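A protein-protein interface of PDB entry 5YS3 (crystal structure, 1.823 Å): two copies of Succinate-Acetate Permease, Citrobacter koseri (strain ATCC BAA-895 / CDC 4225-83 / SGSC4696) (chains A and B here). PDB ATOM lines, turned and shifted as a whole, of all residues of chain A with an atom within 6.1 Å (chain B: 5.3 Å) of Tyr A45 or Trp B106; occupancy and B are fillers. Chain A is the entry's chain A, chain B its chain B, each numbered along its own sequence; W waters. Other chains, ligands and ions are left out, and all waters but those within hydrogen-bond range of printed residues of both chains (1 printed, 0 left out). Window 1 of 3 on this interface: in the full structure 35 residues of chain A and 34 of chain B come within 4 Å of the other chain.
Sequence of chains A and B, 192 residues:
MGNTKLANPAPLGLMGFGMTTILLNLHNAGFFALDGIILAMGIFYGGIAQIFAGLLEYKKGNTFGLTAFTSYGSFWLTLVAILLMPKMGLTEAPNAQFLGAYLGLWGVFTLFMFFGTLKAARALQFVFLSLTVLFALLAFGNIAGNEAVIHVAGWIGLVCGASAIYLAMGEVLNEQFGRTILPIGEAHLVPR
OG of Ser B71 sits at hydrogen-bond distance from OH of Tyr A45 (2.7 Å).
The backbone carbonyl oxygen of Met A41 sits at hydrogen-bond distance from the backbone NH of Gly A46, at 3.0 Å.
O of Phe A44 lies within hydrogen-bond range of N of Ala A49 (2.9 Å).
OG of Ser B74 lies within hydrogen-bond range of O of Thr B70 (2.8 Å).
The backbone carbonyl oxygen (O) of Phe B75 lies within hydrogen-bond range of the side-chain hydroxyl (OG1) of Thr B78 (2.7 Å).
OH of Tyr B102 sits at hydrogen-bond distance from OG1 of Thr B78.
The backbone carbonyl oxygen of Trp B106 lies within hydrogen-bond range of the side-chain hydroxyl of Thr B110 (2.8 Å).
Ser B71 touches Leu A12 (OG to CD1, 3.6 Å).
Met A15 touches Phe B109.
Met A19 touches Leu B105.
Met A19 touches Trp B106.
Phe B109 touches Met A19 (CB to CE, 3.6 Å).
CD2 of Leu A23 touches CD1 of Leu B105 (3.7 Å).
Met A41 touches Thr B78.
Tyr B102 touches Met A41 (CE1 to SD, 3.8 Å).
Thr B78 touches Phe A44 (CG2 to CB, 3.8 Å).
Ser B74 touches Tyr A45.
Of chain B, only Ser B71, Ser B74 and Trp B106 come within 4 Å of Tyr A45.
Printed residues of chain A within 4 Å of Trp B106: Met A19, Met A41 and Tyr A45.
Of the printed residues of chain B, Met A41 touches Thr B78, Tyr B102 and Trp B106.
Of the printed residues of chain B, Leu A23 touches Tyr B102 and Leu B105.
The nearest residue of chain A that does not touch Trp B106 is Leu A23 (6.0 Å).
Printed residues of chain B that touch a printed residue of chain A: Thr B70, Ser B71, Ser B74, Thr B78, Tyr B102, Leu B105, Trp B106 and Phe B109.
Along chain B the printed residues that touch a printed residue of chain A span positions 70 to 109.
Of the 21 printed residues of chain A, 9 touch a printed residue of chain B.
Among the printed residues, no Asp or Glu carboxylate lies within 4 Å of a Lys or Arg side-chain nitrogen of the other chain.
No position is printed for both chains.
Of the 18 pairs that touch across the chains among the printed residues, none has its exchanged pair printed and touching as well.
Water W1 lies within hydrogen-bond range of the backbone carbonyl oxygen of Phe A44 (2.7 Å) and the side-chain hydroxyl of Ser B74 (2.8 Å).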
ATOM      1  N   PRO A  11      26.408 -20.996  15.790  1.00  0.00           N
ATOM      2  CA  PRO A  11      25.124 -20.563  16.341  1.00  0.00           C
ATOM      3  C   PRO A  11      25.287 -19.713  17.591  1.00  0.00           C
ATOM      4  O   PRO A  11      24.557 -18.745  17.760  1.00  0.00           O
ATOM      5  CB  PRO A  11      24.436 -21.883  16.667  1.00  0.00           C
ATOM      6  CG  PRO A  11      24.950 -22.796  15.593  1.00  0.00           C
ATOM      7  CD  PRO A  11      26.410 -22.454  15.562  1.00  0.00           C
ATOM      8  N   LEU A  12      26.224 -20.089  18.459  1.00  0.00           N
ATOM      9  CA  LEU A  12      26.496 -19.292  19.642  1.00  0.00           C
ATOM     10  C   LEU A  12      26.868 -17.869  19.272  1.00  0.00           C
ATOM     11  O   LEU A  12      26.284 -16.918  19.798  1.00  0.00           O
ATOM     12  CB  LEU A  12      27.623 -19.909  20.476  1.00  0.00           C
ATOM     13  CG  LEU A  12      28.056 -19.080  21.702  1.00  0.00           C
ATOM     14  CD1 LEU A  12      26.944 -18.986  22.738  1.00  0.00           C
ATOM     15  CD2 LEU A  12      29.329 -19.657  22.338  1.00  0.00           C
ATOM     16  N   GLY A  13      27.862 -17.723  18.394  1.00  0.00           N
ATOM     17  CA  GLY A  13      28.296 -16.406  17.951  1.00  0.00           C
ATOM     18  C   GLY A  13      27.187 -15.600  17.288  1.00  0.00           C
ATOM     19  O   GLY A  13      27.012 -14.405  17.566  1.00  0.00           O
ATOM     20  N   MET A  15      23.928 -16.015  17.645  1.00  0.00           N
ATOM     21  CA  MET A  15      22.904 -15.671  18.630  1.00  0.00           C
ATOM     22  C   MET A  15      23.297 -14.462  19.459  1.00  0.00           C
ATOM     23  O   MET A  15      22.467 -13.588  19.715  1.00  0.00           O
ATOM     24  CB  MET A  15      22.615 -16.835  19.583  1.00  0.00           C
ATOM     25  CG  MET A  15      21.740 -17.947  18.975  1.00  0.00           C
ATOM     26  SD  MET A  15      20.141 -17.337  18.401  1.00  0.00           S
ATOM     27  CE  MET A  15      19.549 -16.391  19.814  1.00  0.00           C
ATOM     28  N   GLY A  16      24.551 -14.436  19.906  1.00  0.00           N
ATOM     29  CA  GLY A  16      25.037 -13.343  20.723  1.00  0.00           C
ATOM     30  C   GLY A  16      24.979 -12.067  19.902  1.00  0.00           C
ATOM     31  O   GLY A  16      24.465 -11.040  20.350  1.00  0.00           O
ATOM     32  N   PHE A  17      25.485 -12.147  18.676  1.00  0.00           N
ATOM     33  CA  PHE A  17      25.418 -11.007  17.767  1.00  0.00           C
ATOM     34  C   PHE A  17      23.967 -10.590  17.519  1.00  0.00           C
ATOM     35  O   PHE A  17      23.631  -9.416  17.623  1.00  0.00           O
ATOM     36  CB  PHE A  17      26.104 -11.335  16.430  1.00  0.00           C
ATOM     37  CG  PHE A  17      25.784 -10.345  15.340  1.00  0.00           C
ATOM     38  CD1 PHE A  17      26.476  -9.138  15.257  1.00  0.00           C
ATOM     39  CD2 PHE A  17      24.782 -10.595  14.434  1.00  0.00           C
ATOM     40  CE1 PHE A  17      26.175  -8.214  14.267  1.00  0.00           C
ATOM     41  CE2 PHE A  17      24.474  -9.671  13.435  1.00  0.00           C
ATOM     42  CZ  PHE A  17      25.166  -8.486  13.363  1.00  0.00           C
ATOM     43  N   MET A  19      20.826 -11.244  18.988  1.00  0.00           N
ATOM     44  CA  MET A  19      20.060 -10.699  20.106  1.00  0.00           C
ATOM     45  C   MET A  19      20.471  -9.301  20.492  1.00  0.00           C
ATOM     46  O   MET A  19      19.632  -8.436  20.733  1.00  0.00           O
ATOM     47  CB  MET A  19      20.203 -11.581  21.344  1.00  0.00           C
ATOM     48  CG  MET A  19      19.166 -12.638  21.454  1.00  0.00           C
ATOM     49  SD  MET A  19      18.872 -13.126  23.175  1.00  0.00           S
ATOM     50  CE  MET A  19      18.453 -14.801  22.806  1.00  0.00           C
ATOM     51  N   THR A  20      21.780  -9.099  20.586  1.00  0.00           N
ATOM     52  CA  THR A  20      22.316  -7.835  21.036  1.00  0.00           C
ATOM     53  C   THR A  20      22.064  -6.771  19.972  1.00  0.00           C
ATOM     54  O   THR A  20      21.744  -5.630  20.288  1.00  0.00           O
ATOM     55  CB  THR A  20      23.819  -7.952  21.343  1.00  0.00           C
ATOM     56  OG1 THR A  20      24.032  -9.054  22.265  1.00  0.00           O
ATOM     57  CG2 THR A  20      24.331  -6.668  21.963  1.00  0.00           C
ATOM     58  N   LEU A  23      18.390  -5.621  20.298  1.00  0.00           N
ATOM     59  CA  LEU A  23      18.156  -4.720  21.425  1.00  0.00           C
ATOM     60  C   LEU A  23      18.758  -3.340  21.176  1.00  0.00           C
ATOM     61  O   LEU A  23      18.133  -2.317  21.492  1.00  0.00           O
ATOM     62  CB  LEU A  23      18.704  -5.311  22.737  1.00  0.00           C
ATOM     63  CG  LEU A  23      17.995  -6.615  23.109  1.00  0.00           C
ATOM     64  CD1 LEU A  23      18.810  -7.411  24.156  1.00  0.00           C
ATOM     65  CD2 LEU A  23      16.556  -6.357  23.618  1.00  0.00           C
ATOM     66  N   ALA A  40      24.510  -4.589  29.162  1.00  0.00           N
ATOM     67  CA  ALA A  40      24.719  -5.906  29.753  1.00  0.00           C
ATOM     68  C   ALA A  40      24.881  -6.954  28.662  1.00  0.00           C
ATOM     69  O   ALA A  40      25.819  -7.761  28.683  1.00  0.00           O
ATOM     70  CB  ALA A  40      23.539  -6.275  30.683  1.00  0.00           C
ATOM     71  N   MET A  41      23.968  -6.926  27.698  1.00  0.00           N
ATOM     72  CA  MET A  41      24.009  -7.879  26.601  1.00  0.00           C
ATOM     73  C   MET A  41      25.276  -7.665  25.757  1.00  0.00           C
ATOM     74  O   MET A  41      25.936  -8.623  25.366  1.00  0.00           O
ATOM     75  CB  MET A  41      22.739  -7.776  25.745  1.00  0.00           C
ATOM     76  CG  MET A  41      21.501  -8.420  26.391  1.00  0.00           C
ATOM     77  SD  MET A  41      21.454 -10.215  26.267  1.00  0.00           S
ATOM     78  CE  MET A  41      20.754 -10.432  24.639  1.00  0.00           C
ATOM     79  N   GLY A  42      25.655  -6.409  25.537  1.00  0.00           N
ATOM     80  CA  GLY A  42      26.879  -6.132  24.807  1.00  0.00           C
ATOM     81  C   GLY A  42      28.117  -6.712  25.489  1.00  0.00           C
ATOM     82  O   GLY A  42      29.030  -7.185  24.832  1.00  0.00           O
ATOM     83  N   ILE A  43      28.149  -6.675  26.816  1.00  0.00           N
ATOM     84  CA  ILE A  43      29.287  -7.214  27.552  1.00  0.00           C
ATOM     85  C   ILE A  43      29.388  -8.740  27.434  1.00  0.00           C
ATOM     86  O   ILE A  43      30.445  -9.273  27.068  1.00  0.00           O
ATOM     87  CB  ILE A  43      29.230  -6.841  29.060  1.00  0.00           C
ATOM     88  CG1 ILE A  43      29.464  -5.335  29.250  1.00  0.00           C
ATOM     89  CG2 ILE A  43      30.291  -7.625  29.841  1.00  0.00           C
ATOM     90  CD1 ILE A  43      29.136  -4.824  30.657  1.00  0.00           C
ATOM     91  N   PHE A  44      28.297  -9.446  27.725  1.00  0.00           N
ATOM     92  CA  PHE A  44      28.409 -10.880  27.983  1.00  0.00           C
ATOM     93  C   PHE A  44      28.036 -11.779  26.805  1.00  0.00           C
ATOM     94  O   PHE A  44      28.626 -12.847  26.626  1.00  0.00           O
ATOM     95  CB  PHE A  44      27.562 -11.249  29.206  1.00  0.00           C
ATOM     96  CG  PHE A  44      28.124 -10.709  30.489  1.00  0.00           C
ATOM     97  CD1 PHE A  44      29.291 -11.239  31.019  1.00  0.00           C
ATOM     98  CD2 PHE A  44      27.536  -9.622  31.114  1.00  0.00           C
ATOM     99  CE1 PHE A  44      29.833 -10.731  32.191  1.00  0.00           C
ATOM    100  CE2 PHE A  44      28.070  -9.104  32.279  1.00  0.00           C
ATOM    101  CZ  PHE A  44      29.213  -9.656  32.825  1.00  0.00           C
ATOM    102  N   TYR A  45      27.065 -11.354  26.011  1.00  0.00           N
ATOM    103  CA  TYR A  45      26.516 -12.213  24.973  1.00  0.00           C
ATOM    104  C   TYR A  45      26.980 -11.765  23.585  1.00  0.00           C
ATOM    105  O   TYR A  45      27.624 -12.530  22.873  1.00  0.00           O
ATOM    106  CB  TYR A  45      24.987 -12.221  25.057  1.00  0.00           C
ATOM    107  CG  TYR A  45      24.333 -13.432  24.437  1.00  0.00           C
ATOM    108  CD1 TYR A  45      24.957 -14.682  24.458  1.00  0.00           C
ATOM    109  CD2 TYR A  45      23.071 -13.338  23.853  1.00  0.00           C
ATOM    110  CE1 TYR A  45      24.345 -15.785  23.902  1.00  0.00           C
ATOM    111  CE2 TYR A  45      22.465 -14.433  23.294  1.00  0.00           C
ATOM    112  CZ  TYR A  45      23.100 -15.652  23.315  1.00  0.00           C
ATOM    113  OH  TYR A  45      22.459 -16.743  22.763  1.00  0.00           O
ATOM    114  N   GLY A  46      26.658 -10.535  23.195  1.00  0.00           N
ATOM    115  CA  GLY A  46      27.227  -9.993  21.968  1.00  0.00           C
ATOM    116  C   GLY A  46      28.736  -9.915  22.110  1.00  0.00           C
ATOM    117  O   GLY A  46      29.489 -10.055  21.142  1.00  0.00           O
ATOM    118  N   GLY A  47      29.189  -9.695  23.334  1.00  0.00           N
ATOM    119  CA  GLY A  47      30.610  -9.552  23.586  1.00  0.00           C
ATOM    120  C   GLY A  47      31.339 -10.855  23.854  1.00  0.00           C
ATOM    121  O   GLY A  47      31.804 -11.522  22.931  1.00  0.00           O
ATOM    122  N   ILE A  48      31.439 -11.219  25.127  1.00  0.00           N
ATOM    123  CA  ILE A  48      32.263 -12.358  25.536  1.00  0.00           C
ATOM    124  C   ILE A  48      31.868 -13.701  24.891  1.00  0.00           C
ATOM    125  O   ILE A  48      32.742 -14.444  24.401  1.00  0.00           O
ATOM    126  CB  ILE A  48      32.251 -12.493  27.081  1.00  0.00           C
ATOM    127  CG1 ILE A  48      33.051 -11.337  27.694  1.00  0.00           C
ATOM    128  CG2 ILE A  48      32.828 -13.847  27.504  1.00  0.00           C
ATOM    129  CD1 ILE A  48      32.806 -11.121  29.180  1.00  0.00           C
ATOM    130  N   ALA A  49      30.578 -14.028  24.880  1.00  0.00           N
ATOM    131  CA  ALA A  49      30.157 -15.292  24.283  1.00  0.00           C
ATOM    132  C   ALA A  49      30.515 -15.348  22.795  1.00  0.00           C
ATOM    133  O   ALA A  49      30.858 -16.412  22.274  1.00  0.00           O
ATOM    134  CB  ALA A  49      28.663 -15.518  24.466  1.00  0.00           C
ATOM    135  N   GLN A  50      30.440 -14.207  22.112  1.00  0.00           N
ATOM    136  CA  GLN A  50      30.811 -14.179  20.708  1.00  0.00           C
ATOM    137  C   GLN A  50      32.330 -14.352  20.560  1.00  0.00           C
ATOM    138  O   GLN A  50      32.799 -14.973  19.619  1.00  0.00           O
ATOM    139  CB  GLN A  50      30.335 -12.886  20.030  1.00  0.00           C
ATOM    140  CG  GLN A  50      30.513 -12.933  18.545  1.00  0.00           C
ATOM    141  CD  GLN A  50      29.768 -11.835  17.775  1.00  0.00           C
ATOM    142  OE1 GLN A  50      29.241 -10.855  18.334  1.00  0.00           O
ATOM    143  NE2 GLN A  50      29.739 -12.000  16.488  1.00  0.00           N
ATOM    144  N   ILE A  51      33.103 -13.819  21.501  1.00  0.00           N
ATOM    145  CA  ILE A  51      34.542 -14.044  21.475  1.00  0.00           C
ATOM    146  C   ILE A  51      34.856 -15.540  21.660  1.00  0.00           C
ATOM    147  O   ILE A  51      35.685 -16.087  20.937  1.00  0.00           O
ATOM    148  CB  ILE A  51      35.250 -13.172  22.534  1.00  0.00           C
ATOM    149  CG1 ILE A  51      35.235 -11.715  22.055  1.00  0.00           C
ATOM    150  CG2 ILE A  51      36.691 -13.645  22.785  1.00  0.00           C
ATOM    151  CD1 ILE A  51      35.738 -10.712  23.044  1.00  0.00           C
ATOM    152  N   THR B  70      26.091 -22.165  27.055  1.00  0.00           N
ATOM    153  CA  THR B  70      26.879 -20.920  27.004  1.00  0.00           C
ATOM    154  C   THR B  70      25.951 -19.703  26.894  1.00  0.00           C
ATOM    155  O   THR B  70      26.211 -18.644  27.486  1.00  0.00           O
ATOM    156  CB  THR B  70      27.889 -20.930  25.828  1.00  0.00           C
ATOM    157  OG1 THR B  70      28.589 -22.191  25.818  1.00  0.00           O
ATOM    158  CG2 THR B  70      28.914 -19.825  26.005  1.00  0.00           C
ATOM    159  N   SER B  71      24.866 -19.854  26.143  1.00  0.00           N
ATOM    160  CA  SER B  71      23.875 -18.774  26.012  1.00  0.00           C
ATOM    161  C   SER B  71      23.128 -18.496  27.333  1.00  0.00           C
ATOM    162  O   SER B  71      23.003 -17.338  27.762  1.00  0.00           O
ATOM    163  CB  SER B  71      22.850 -19.105  24.913  1.00  0.00           C
ATOM    164  OG  SER B  71      23.450 -19.128  23.630  1.00  0.00           O
ATOM    165  N   TYR B  72      22.631 -19.539  27.985  1.00  0.00           N
ATOM    166  CA  TYR B  72      21.854 -19.293  29.194  1.00  0.00           C
ATOM    167  C   TYR B  72      22.771 -18.883  30.339  1.00  0.00           C
ATOM    168  O   TYR B  72      22.366 -18.124  31.219  1.00  0.00           O
ATOM    169  CB  TYR B  72      20.997 -20.518  29.573  1.00  0.00           C
ATOM    170  CG  TYR B  72      19.874 -20.758  28.603  1.00  0.00           C
ATOM    171  CD1 TYR B  72      18.921 -19.765  28.348  1.00  0.00           C
ATOM    172  CD2 TYR B  72      19.759 -21.967  27.935  1.00  0.00           C
ATOM    173  CE1 TYR B  72      17.884 -19.981  27.444  1.00  0.00           C
ATOM    174  CE2 TYR B  72      18.722 -22.197  27.045  1.00  0.00           C
ATOM    175  CZ  TYR B  72      17.786 -21.198  26.806  1.00  0.00           C
ATOM    176  OH  TYR B  72      16.757 -21.448  25.913  1.00  0.00           O
ATOM    177  N   SER B  74      25.310 -16.952  29.768  1.00  0.00           N
ATOM    178  CA  SER B  74      25.411 -15.535  29.440  1.00  0.00           C
ATOM    179  C   SER B  74      24.157 -14.774  29.879  1.00  0.00           C
ATOM    180  O   SER B  74      24.245 -13.661  30.392  1.00  0.00           O
ATOM    181  CB  SER B  74      25.655 -15.357  27.940  1.00  0.00           C
ATOM    182  OG  SER B  74      26.917 -15.909  27.607  1.00  0.00           O
ATOM    183  N   PHE B  75      22.996 -15.364  29.672  1.00  0.00           N
ATOM    184  CA  PHE B  75      21.748 -14.739  30.140  1.00  0.00           C
ATOM    185  C   PHE B  75      21.799 -14.350  31.614  1.00  0.00           C
ATOM    186  O   PHE B  75      21.456 -13.226  31.986  1.00  0.00           O
ATOM    187  CB  PHE B  75      20.560 -15.658  29.937  1.00  0.00           C
ATOM    188  CG  PHE B  75      19.364 -15.255  30.759  1.00  0.00           C
ATOM    189  CD1 PHE B  75      18.549 -14.217  30.340  1.00  0.00           C
ATOM    190  CD2 PHE B  75      19.071 -15.899  31.950  1.00  0.00           C
ATOM    191  CE1 PHE B  75      17.469 -13.831  31.107  1.00  0.00           C
ATOM    192  CE2 PHE B  75      17.995 -15.516  32.716  1.00  0.00           C
ATOM    193  CZ  PHE B  75      17.198 -14.475  32.296  1.00  0.00           C
ATOM    194  N   THR B  78      23.953 -11.416  32.166  1.00  0.00           N
ATOM    195  CA  THR B  78      23.362 -10.158  31.694  1.00  0.00           C
ATOM    196  C   THR B  78      22.295  -9.677  32.682  1.00  0.00           C
ATOM    197  O   THR B  78      22.212  -8.494  32.971  1.00  0.00           O
ATOM    198  CB  THR B  78      22.729 -10.278  30.280  1.00  0.00           C
ATOM    199  OG1 THR B  78      21.602 -11.164  30.304  1.00  0.00           O
ATOM    200  CG2 THR B  78      23.762 -10.796  29.263  1.00  0.00           C
ATOM    201  N   ALA B 101      11.039  -6.945  26.299  1.00  0.00           N
ATOM    202  CA  ALA B 101      11.509  -7.293  24.954  1.00  0.00           C
ATOM    203  C   ALA B 101      12.677  -8.278  25.060  1.00  0.00           C
ATOM    204  O   ALA B 101      12.736  -9.280  24.354  1.00  0.00           O
ATOM    205  CB  ALA B 101      11.936  -6.037  24.186  1.00  0.00           C
ATOM    206  N   TYR B 102      13.599  -7.950  25.955  1.00  0.00           N
ATOM    207  CA  TYR B 102      14.807  -8.744  26.222  1.00  0.00           C
ATOM    208  C   TYR B 102      14.404 -10.140  26.639  1.00  0.00           C
ATOM    209  O   TYR B 102      14.890 -11.116  26.096  1.00  0.00           O
ATOM    210  CB  TYR B 102      15.636  -8.003  27.281  1.00  0.00           C
ATOM    211  CG  TYR B 102      16.547  -8.776  28.231  1.00  0.00           C
ATOM    212  CD1 TYR B 102      17.889  -9.016  27.917  1.00  0.00           C
ATOM    213  CD2 TYR B 102      16.095  -9.162  29.486  1.00  0.00           C
ATOM    214  CE1 TYR B 102      18.735  -9.665  28.816  1.00  0.00           C
ATOM    215  CE2 TYR B 102      16.933  -9.812  30.393  1.00  0.00           C
ATOM    216  CZ  TYR B 102      18.241 -10.068  30.053  1.00  0.00           C
ATOM    217  OH  TYR B 102      19.057 -10.701  30.955  1.00  0.00           O
ATOM    218  N   LEU B 103      13.451 -10.241  27.562  1.00  0.00           N
ATOM    219  CA  LEU B 103      12.970 -11.555  27.970  1.00  0.00           C
ATOM    220  C   LEU B 103      12.276 -12.290  26.821  1.00  0.00           C
ATOM    221  O   LEU B 103      12.377 -13.516  26.694  1.00  0.00           O
ATOM    222  CB  LEU B 103      12.029 -11.418  29.181  1.00  0.00           C
ATOM    223  CG  LEU B 103      12.814 -10.998  30.426  1.00  0.00           C
ATOM    224  CD1 LEU B 103      11.925 -10.479  31.549  1.00  0.00           C
ATOM    225  CD2 LEU B 103      13.666 -12.168  30.919  1.00  0.00           C
ATOM    226  N   GLY B 104      11.580 -11.549  25.967  1.00  0.00           N
ATOM    227  CA  GLY B 104      10.913 -12.177  24.840  1.00  0.00           C
ATOM    228  C   GLY B 104      11.883 -12.795  23.850  1.00  0.00           C
ATOM    229  O   GLY B 104      11.623 -13.858  23.299  1.00  0.00           O
ATOM    230  N   LEU B 105      13.002 -12.117  23.619  1.00  0.00           N
ATOM    231  CA  LEU B 105      14.044 -12.634  22.737  1.00  0.00           C
ATOM    232  C   LEU B 105      14.610 -13.938  23.304  1.00  0.00           C
ATOM    233  O   LEU B 105      14.846 -14.890  22.566  1.00  0.00           O
ATOM    234  CB  LEU B 105      15.169 -11.605  22.560  1.00  0.00           C
ATOM    235  CG  LEU B 105      14.918 -10.420  21.628  1.00  0.00           C
ATOM    236  CD1 LEU B 105      16.087  -9.437  21.615  1.00  0.00           C
ATOM    237  CD2 LEU B 105      14.674 -10.957  20.227  1.00  0.00           C
ATOM    238  N   TRP B 106      14.835 -13.972  24.615  1.00  0.00           N
ATOM    239  CA  TRP B 106      15.335 -15.197  25.241  1.00  0.00           C
ATOM    240  C   TRP B 106      14.307 -16.303  25.087  1.00  0.00           C
ATOM    241  O   TRP B 106      14.659 -17.467  24.878  1.00  0.00           O
ATOM    242  CB  TRP B 106      15.695 -14.951  26.727  1.00  0.00           C
ATOM    243  CG  TRP B 106      17.002 -14.270  26.826  1.00  0.00           C
ATOM    244  CD1 TRP B 106      17.231 -12.949  27.082  1.00  0.00           C
ATOM    245  CD2 TRP B 106      18.288 -14.871  26.603  1.00  0.00           C
ATOM    246  NE1 TRP B 106      18.582 -12.696  27.041  1.00  0.00           N
ATOM    247  CE2 TRP B 106      19.248 -13.859  26.753  1.00  0.00           C
ATOM    248  CE3 TRP B 106      18.709 -16.168  26.298  1.00  0.00           C
ATOM    249  CZ2 TRP B 106      20.624 -14.104  26.602  1.00  0.00           C
ATOM    250  CZ3 TRP B 106      20.066 -16.408  26.158  1.00  0.00           C
ATOM    251  CH2 TRP B 106      21.005 -15.380  26.310  1.00  0.00           C
ATOM    252  N   GLY B 107      13.025 -15.938  25.175  1.00  0.00           N
ATOM    253  CA  GLY B 107      11.962 -16.903  24.954  1.00  0.00           C
ATOM    254  C   GLY B 107      11.916 -17.426  23.532  1.00  0.00           C
ATOM    255  O   GLY B 107      11.684 -18.616  23.293  1.00  0.00           O
ATOM    256  N   VAL B 108      12.124 -16.535  22.566  1.00  0.00           N
ATOM    257  CA  VAL B 108      12.136 -16.958  21.166  1.00  0.00           C
ATOM    258  C   VAL B 108      13.281 -17.941  20.909  1.00  0.00           C
ATOM    259  O   VAL B 108      13.107 -18.970  20.255  1.00  0.00           O
ATOM    260  CB  VAL B 108      12.266 -15.748  20.215  1.00  0.00           C
ATOM    261  CG1 VAL B 108      12.648 -16.201  18.814  1.00  0.00           C
ATOM    262  CG2 VAL B 108      10.960 -14.934  20.211  1.00  0.00           C
ATOM    263  N   PHE B 109      14.460 -17.601  21.417  1.00  0.00           N
ATOM    264  CA  PHE B 109      15.600 -18.512  21.387  1.00  0.00           C
ATOM    265  C   PHE B 109      15.203 -19.857  21.991  1.00  0.00           C
ATOM    266  O   PHE B 109      15.417 -20.904  21.393  1.00  0.00           O
ATOM    267  CB  PHE B 109      16.769 -17.893  22.154  1.00  0.00           C
ATOM    268  CG  PHE B 109      17.916 -18.831  22.422  1.00  0.00           C
ATOM    269  CD1 PHE B 109      18.643 -19.383  21.371  1.00  0.00           C
ATOM    270  CD2 PHE B 109      18.305 -19.120  23.737  1.00  0.00           C
ATOM    271  CE1 PHE B 109      19.736 -20.220  21.616  1.00  0.00           C
ATOM    272  CE2 PHE B 109      19.394 -19.956  23.987  1.00  0.00           C
ATOM    273  CZ  PHE B 109      20.108 -20.513  22.928  1.00  0.00           C
ATOM    274  N   THR B 110      14.583 -19.814  23.164  1.00  0.00           N
ATOM    275  CA  THR B 110      14.223 -21.055  23.852  1.00  0.00           C
ATOM    276  C   THR B 110      13.223 -21.895  23.049  1.00  0.00           C
ATOM    277  O   THR B 110      13.324 -23.120  23.027  1.00  0.00           O
ATOM    278  CB  THR B 110      13.646 -20.768  25.258  1.00  0.00           C
ATOM    279  OG1 THR B 110      14.591 -19.993  26.000  1.00  0.00           O
ATOM    280  CG2 THR B 110      13.414 -22.072  26.009  1.00  0.00           C
ATOM    281  N   LEU B 111      12.263 -21.238  22.392  1.00  0.00           N
ATOM    282  CA  LEU B 111      11.298 -21.970  21.558  1.00  0.00           C
ATOM    283  C   LEU B 111      11.936 -22.677  20.369  1.00  0.00           C
ATOM    284  O   LEU B 111      11.616 -23.831  20.091  1.00  0.00           O
ATOM    285  CB  LEU B 111      10.206 -21.027  21.051  1.00  0.00           C
ATOM    286  CG  LEU B 111       9.134 -21.625  20.132  1.00  0.00           C
ATOM    287  CD1 LEU B 111       8.384 -22.770  20.788  1.00  0.00           C
ATOM    288  CD2 LEU B 111       8.175 -20.528  19.756  1.00  0.00           C
ATOM    289  N   PHE B 135       9.722 -17.732  30.034  1.00  0.00           N
ATOM    290  CA  PHE B 135      10.174 -16.477  29.436  1.00  0.00           C
ATOM    291  C   PHE B 135       8.985 -15.695  28.870  1.00  0.00           C
ATOM    292  O   PHE B 135       8.914 -14.483  29.026  1.00  0.00           O
ATOM    293  CB  PHE B 135      11.211 -16.721  28.340  1.00  0.00           C
ATOM    294  CG  PHE B 135      12.629 -16.836  28.847  1.00  0.00           C
ATOM    295  CD1 PHE B 135      13.214 -15.785  29.540  1.00  0.00           C
ATOM    296  CD2 PHE B 135      13.377 -17.975  28.600  1.00  0.00           C
ATOM    297  CE1 PHE B 135      14.528 -15.866  29.994  1.00  0.00           C
ATOM    298  CE2 PHE B 135      14.690 -18.073  29.047  1.00  0.00           C
ATOM    299  CZ  PHE B 135      15.271 -17.013  29.751  1.00  0.00           C
HETATM  300  O   HOH W   1      29.222 -14.619  28.612  1.00  0.00           O
